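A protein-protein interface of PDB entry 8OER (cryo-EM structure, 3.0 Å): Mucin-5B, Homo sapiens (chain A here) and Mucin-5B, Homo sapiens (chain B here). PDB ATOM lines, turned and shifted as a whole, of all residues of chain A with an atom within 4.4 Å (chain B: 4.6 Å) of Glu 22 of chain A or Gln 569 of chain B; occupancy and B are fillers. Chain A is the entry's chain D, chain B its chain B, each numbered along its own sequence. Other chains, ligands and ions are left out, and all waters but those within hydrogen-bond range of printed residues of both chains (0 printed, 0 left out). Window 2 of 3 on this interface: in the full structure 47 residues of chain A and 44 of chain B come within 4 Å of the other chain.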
ATOM      1  N   PRO A  19      28.927  12.425 -31.094  1.00  0.00           N
ATOM      2  CA  PRO A  19      29.416  11.141 -30.577  1.00  0.00           C
ATOM      3  C   PRO A  19      29.613  11.171 -29.072  1.00  0.00           C
ATOM      4  O   PRO A  19      30.499  11.864 -28.566  1.00  0.00           O
ATOM      5  CB  PRO A  19      30.750  10.946 -31.312  1.00  0.00           C
ATOM      6  CG  PRO A  19      30.716  11.910 -32.458  1.00  0.00           C
ATOM      7  CD  PRO A  19      29.902  13.065 -31.988  1.00  0.00           C
ATOM      8  N   GLY A  20      28.795  10.420 -28.351  1.00  0.00           N
ATOM      9  CA  GLY A  20      28.845  10.383 -26.905  1.00  0.00           C
ATOM     10  C   GLY A  20      29.925   9.465 -26.386  1.00  0.00           C
ATOM     11  O   GLY A  20      30.885   9.134 -27.087  1.00  0.00           O
ATOM     12  N   ALA A  21      29.767   9.046 -25.130  1.00  0.00           N
ATOM     13  CA  ALA A  21      30.762   8.174 -24.521  1.00  0.00           C
ATOM     14  C   ALA A  21      30.791   6.806 -25.183  1.00  0.00           C
ATOM     15  O   ALA A  21      31.768   6.065 -25.030  1.00  0.00           O
ATOM     16  CB  ALA A  21      30.498   8.037 -23.022  1.00  0.00           C
ATOM     17  N   GLU A  22      29.730   6.441 -25.906  1.00  0.00           N
ATOM     18  CA  GLU A  22      29.760   5.188 -26.651  1.00  0.00           C
ATOM     19  C   GLU A  22      30.772   5.264 -27.786  1.00  0.00           C
ATOM     20  O   GLU A  22      31.490   4.293 -28.050  1.00  0.00           O
ATOM     21  CB  GLU A  22      28.362   4.838 -27.171  1.00  0.00           C
ATOM     22  CG  GLU A  22      27.947   5.513 -28.471  1.00  0.00           C
ATOM     23  CD  GLU A  22      27.863   7.021 -28.354  1.00  0.00           C
ATOM     24  OE1 GLU A  22      27.598   7.516 -27.241  1.00  0.00           O
ATOM     25  OE2 GLU A  22      28.070   7.715 -29.369  1.00  0.00           O
ATOM     26  N   CYS A  23      30.863   6.414 -28.445  1.00  0.00           N
ATOM     27  CA  CYS A  23      31.861   6.632 -29.486  1.00  0.00           C
ATOM     28  C   CYS A  23      33.130   7.219 -28.885  1.00  0.00           C
ATOM     29  O   CYS A  23      33.683   8.212 -29.352  1.00  0.00           O
ATOM     30  CB  CYS A  23      31.289   7.542 -30.565  1.00  0.00           C
ATOM     31  SG  CYS A  23      30.018   6.774 -31.588  1.00  0.00           S
ATOM     32  N   LEU A  24      33.592   6.576 -27.820  1.00  0.00           N
ATOM     33  CA  LEU A  24      34.795   7.000 -27.125  1.00  0.00           C
ATOM     34  C   LEU A  24      36.009   6.502 -27.886  1.00  0.00           C
ATOM     35  O   LEU A  24      36.075   5.327 -28.258  1.00  0.00           O
ATOM     36  CB  LEU A  24      34.784   6.457 -25.697  1.00  0.00           C
ATOM     37  CG  LEU A  24      35.963   6.561 -24.722  1.00  0.00           C
ATOM     38  CD1 LEU A  24      36.818   5.311 -24.817  1.00  0.00           C
ATOM     39  CD2 LEU A  24      36.799   7.813 -24.923  1.00  0.00           C
ATOM     40  N   THR A  29      38.077   1.155 -31.046  1.00  0.00           N
ATOM     41  CA  THR A  29      37.244   2.015 -31.871  1.00  0.00           C
ATOM     42  C   THR A  29      37.997   3.228 -32.398  1.00  0.00           C
ATOM     43  O   THR A  29      37.428   4.026 -33.151  1.00  0.00           O
ATOM     44  CB  THR A  29      36.000   2.440 -31.088  1.00  0.00           C
ATOM     45  OG1 THR A  29      35.578   1.349 -30.263  1.00  0.00           O
ATOM     46  CG2 THR A  29      34.857   2.793 -32.032  1.00  0.00           C
ATOM     47  N   CYS A  34      33.261   4.792 -35.005  1.00  0.00           N
ATOM     48  CA  CYS A  34      32.095   4.448 -34.208  1.00  0.00           C
ATOM     49  C   CYS A  34      30.812   4.879 -34.906  1.00  0.00           C
ATOM     50  O   CYS A  34      30.800   5.859 -35.657  1.00  0.00           O
ATOM     51  CB  CYS A  34      32.175   5.089 -32.822  1.00  0.00           C
ATOM     52  SG  CYS A  34      30.690   4.878 -31.829  1.00  0.00           S
ATOM     53  N   PHE A  35      29.737   4.134 -34.657  1.00  0.00           N
ATOM     54  CA  PHE A  35      28.410   4.438 -35.174  1.00  0.00           C
ATOM     55  C   PHE A  35      27.409   4.426 -34.025  1.00  0.00           C
ATOM     56  O   PHE A  35      27.388   3.477 -33.232  1.00  0.00           O
ATOM     57  CB  PHE A  35      27.994   3.432 -36.244  1.00  0.00           C
ATOM     58  CG  PHE A  35      29.030   3.202 -37.301  1.00  0.00           C
ATOM     59  CD1 PHE A  35      29.068   3.994 -38.432  1.00  0.00           C
ATOM     60  CD2 PHE A  35      29.951   2.180 -37.177  1.00  0.00           C
ATOM     61  CE1 PHE A  35      30.012   3.782 -39.409  1.00  0.00           C
ATOM     62  CE2 PHE A  35      30.895   1.964 -38.156  1.00  0.00           C
ATOM     63  CZ  PHE A  35      30.928   2.767 -39.269  1.00  0.00           C
ATOM     64  N   SER A  36      26.587   5.473 -33.940  1.00  0.00           N
ATOM     65  CA  SER A  36      25.505   5.538 -32.962  1.00  0.00           C
ATOM     66  C   SER A  36      24.606   6.718 -33.292  1.00  0.00           C
ATOM     67  O   SER A  36      25.099   7.796 -33.637  1.00  0.00           O
ATOM     68  CB  SER A  36      26.041   5.679 -31.536  1.00  0.00           C
ATOM     69  OG  SER A  36      24.978   5.663 -30.600  1.00  0.00           O
ATOM     70  N   HIS A  38      22.517   7.938 -30.962  1.00  0.00           N
ATOM     71  CA  HIS A  38      22.200   8.575 -29.689  1.00  0.00           C
ATOM     72  C   HIS A  38      23.488   8.869 -28.935  1.00  0.00           C
ATOM     73  O   HIS A  38      24.359   8.001 -28.827  1.00  0.00           O
ATOM     74  CB  HIS A  38      21.285   7.690 -28.842  1.00  0.00           C
ATOM     75  CG  HIS A  38      21.923   6.408 -28.408  1.00  0.00           C
ATOM     76  ND1 HIS A  38      22.342   6.187 -27.113  1.00  0.00           N
ATOM     77  CD2 HIS A  38      22.229   5.285 -29.099  1.00  0.00           C
ATOM     78  CE1 HIS A  38      22.869   4.979 -27.024  1.00  0.00           C
ATOM     79  NE2 HIS A  38      22.815   4.411 -28.214  1.00  0.00           N
ATOM     80  N   CYS A  39      23.608  10.090 -28.422  1.00  0.00           N
ATOM     81  CA  CYS A  39      24.697  10.416 -27.516  1.00  0.00           C
ATOM     82  C   CYS A  39      24.436   9.815 -26.142  1.00  0.00           C
ATOM     83  O   CYS A  39      23.290   9.669 -25.714  1.00  0.00           O
ATOM     84  CB  CYS A  39      24.861  11.927 -27.394  1.00  0.00           C
ATOM     85  SG  CYS A  39      26.091  12.449 -26.172  1.00  0.00           S
ATOM     86  N   VAL A  40      25.516   9.463 -25.446  1.00  0.00           N
ATOM     87  CA  VAL A  40      25.430   8.982 -24.074  1.00  0.00           C
ATOM     88  C   VAL A  40      26.393   9.792 -23.219  1.00  0.00           C
ATOM     89  O   VAL A  40      27.474  10.181 -23.678  1.00  0.00           O
ATOM     90  CB  VAL A  40      25.735   7.472 -23.956  1.00  0.00           C
ATOM     91  CG1 VAL A  40      24.883   6.675 -24.924  1.00  0.00           C
ATOM     92  CG2 VAL A  40      27.197   7.187 -24.159  1.00  0.00           C
ATOM     93  N   CYS B 422      25.842  -6.413 -30.502  1.00  0.00           N
ATOM     94  CA  CYS B 422      26.411  -5.120 -30.871  1.00  0.00           C
ATOM     95  C   CYS B 422      26.026  -4.843 -32.315  1.00  0.00           C
ATOM     96  O   CYS B 422      25.239  -5.583 -32.915  1.00  0.00           O
ATOM     97  CB  CYS B 422      27.925  -5.095 -30.682  1.00  0.00           C
ATOM     98  SG  CYS B 422      28.672  -3.483 -30.961  1.00  0.00           S
ATOM     99  N   LYS B 567      33.411  -4.703 -33.921  1.00  0.00           N
ATOM    100  CA  LYS B 567      32.274  -4.077 -33.262  1.00  0.00           C
ATOM    101  C   LYS B 567      32.242  -2.588 -33.569  1.00  0.00           C
ATOM    102  O   LYS B 567      33.284  -1.947 -33.718  1.00  0.00           O
ATOM    103  CB  LYS B 567      32.347  -4.292 -31.754  1.00  0.00           C
ATOM    104  CG  LYS B 567      32.363  -5.731 -31.341  1.00  0.00           C
ATOM    105  CD  LYS B 567      32.131  -5.853 -29.862  1.00  0.00           C
ATOM    106  CE  LYS B 567      33.236  -5.172 -29.104  1.00  0.00           C
ATOM    107  NZ  LYS B 567      33.231  -5.583 -27.680  1.00  0.00           N
ATOM    108  N   ALA B 568      31.037  -2.036 -33.690  1.00  0.00           N
ATOM    109  CA  ALA B 568      30.935  -0.600 -33.908  1.00  0.00           C
ATOM    110  C   ALA B 568      31.312   0.181 -32.656  1.00  0.00           C
ATOM    111  O   ALA B 568      32.126   1.108 -32.720  1.00  0.00           O
ATOM    112  CB  ALA B 568      29.527  -0.233 -34.366  1.00  0.00           C
ATOM    113  N   GLN B 569      30.755  -0.191 -31.506  1.00  0.00           N
ATOM    114  CA  GLN B 569      30.906   0.569 -30.273  1.00  0.00           C
ATOM    115  C   GLN B 569      31.842  -0.155 -29.318  1.00  0.00           C
ATOM    116  O   GLN B 569      31.661  -1.345 -29.053  1.00  0.00           O
ATOM    117  CB  GLN B 569      29.552   0.777 -29.598  1.00  0.00           C
ATOM    118  CG  GLN B 569      28.603   1.654 -30.370  1.00  0.00           C
ATOM    119  CD  GLN B 569      27.253   1.751 -29.701  1.00  0.00           C
ATOM    120  OE1 GLN B 569      26.843   0.844 -28.983  1.00  0.00           O
ATOM    121  NE2 GLN B 569      26.551   2.852 -29.939  1.00  0.00           N
ATOM    122  N   ALA B 570      32.820   0.575 -28.777  1.00  0.00           N
ATOM    123  CA  ALA B 570      33.726  -0.006 -27.791  1.00  0.00           C
ATOM    124  C   ALA B 570      32.995  -0.512 -26.557  1.00  0.00           C
ATOM    125  O   ALA B 570      33.519  -1.382 -25.853  1.00  0.00           O
ATOM    126  CB  ALA B 570      34.776   1.014 -27.357  1.00  0.00           C
ATOM    127  N   ALA B 571      31.810   0.013 -26.272  1.00  0.00           N
ATOM    128  CA  ALA B 571      31.081  -0.370 -25.074  1.00  0.00           C
ATOM    129  C   ALA B 571      30.323  -1.677 -25.235  1.00  0.00           C
ATOM    130  O   ALA B 571      29.707  -2.136 -24.268  1.00  0.00           O
ATOM    131  CB  ALA B 571      30.110   0.740 -24.671  1.00  0.00           C
ATOM    132  N   CYS B 572      30.348  -2.281 -26.416  1.00  0.00           N
ATOM    133  CA  CYS B 572      29.634  -3.529 -26.615  1.00  0.00           C
ATOM    134  C   CYS B 572      30.308  -4.656 -25.846  1.00  0.00           C
ATOM    135  O   CYS B 572      31.443  -4.540 -25.381  1.00  0.00           O
ATOM    136  CB  CYS B 572      29.558  -3.879 -28.099  1.00  0.00           C
ATOM    137  SG  CYS B 572      28.735  -2.642 -29.119  1.00  0.00           S
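NE2 of Gln 569 of chain B sits at hydrogen-bond distance from O of Phe 35 of chain A (3.5 Å).
The side-chain hydroxyl (OG) of Ser 36 of chain A sits close to the side-chain amide nitrogen (NE2) of Gln 569 of chain B, at 3.3 Å.
The backbone NH of Ala 570 of chain B lies close to the side-chain hydroxyl of Thr 29 of chain A (3.2 Å).
The backbone NH (N) of Gly 20 of chain A lies within hydrogen-bond range of the side-chain carboxylate (OE2) of Glu 22 of chain A, 3.0 Å away.
The side-chain carboxylate (OE1) of Glu 22 of chain A lies close to the backbone NH (N) of Val 40 of chain A, at 3.4 Å.
The side-chain sulfur of Cys 23 of chain A forms a disulfide with the side-chain sulfur of Cys 34 of chain A.
The side-chain hydroxyl of Ser 36 of chain A is in hydrogen-bond range of the backbone carbonyl oxygen of His 38 of chain A, at 3.0 Å.
SG of Cys 422 of chain B forms a disulfide with SG of Cys 572 of chain B (2.0 Å).
CG of Glu 22 of chain A touches NE2 of Gln 569 of chain B, 3.3 Å away.
Ala 568 of chain B touches Thr 29 of chain A (O to CG2, 3.3 Å).
CA of Cys 34 of chain A touches O of Ala 568 of chain B (3.7 Å).
Ala 568 of chain B touches Phe 35 of chain A (CB to CD2, 3.7 Å).
Printed residues of chain B within 4 Å of Glu 22 of chain A: Gln 569 (3.3 Å).
Gln 569 of chain B touches just these residues of chain A: Glu 22, Phe 35 and Ser 36.
Of the printed residues of chain A, Ala 568 of chain B touches Thr 29, Cys 34 and Phe 35.
Printed residues of chain B within 4 Å of Thr 29 of chain A: Ala 568 and Ala 570.
Printed residues of chain B within 4 Å of Ser 36 of chain A: Gln 569 (3.3 Å).
Lys 567 of chain B touches none of the printed residues of chain A.
Cys 39 of chain A touches none of the printed residues of chain B.
The nearest printed residue of chain B that does not touch Glu 22 of chain A is Ala 570 of chain B (4.02 Å).
Printed residues of chain A that touch a printed residue of chain B: Glu 22, Thr 29, Cys 34, Phe 35 and Ser 36.
Hydrophobic or aromatic side chains of chain A within 4 Å of the printed part of chain B: Phe 35.
Along chain A the printed residues that touch a printed residue of chain B span positions 22 to 36.
Among the printed residues, 7 pairs touch across the chains.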
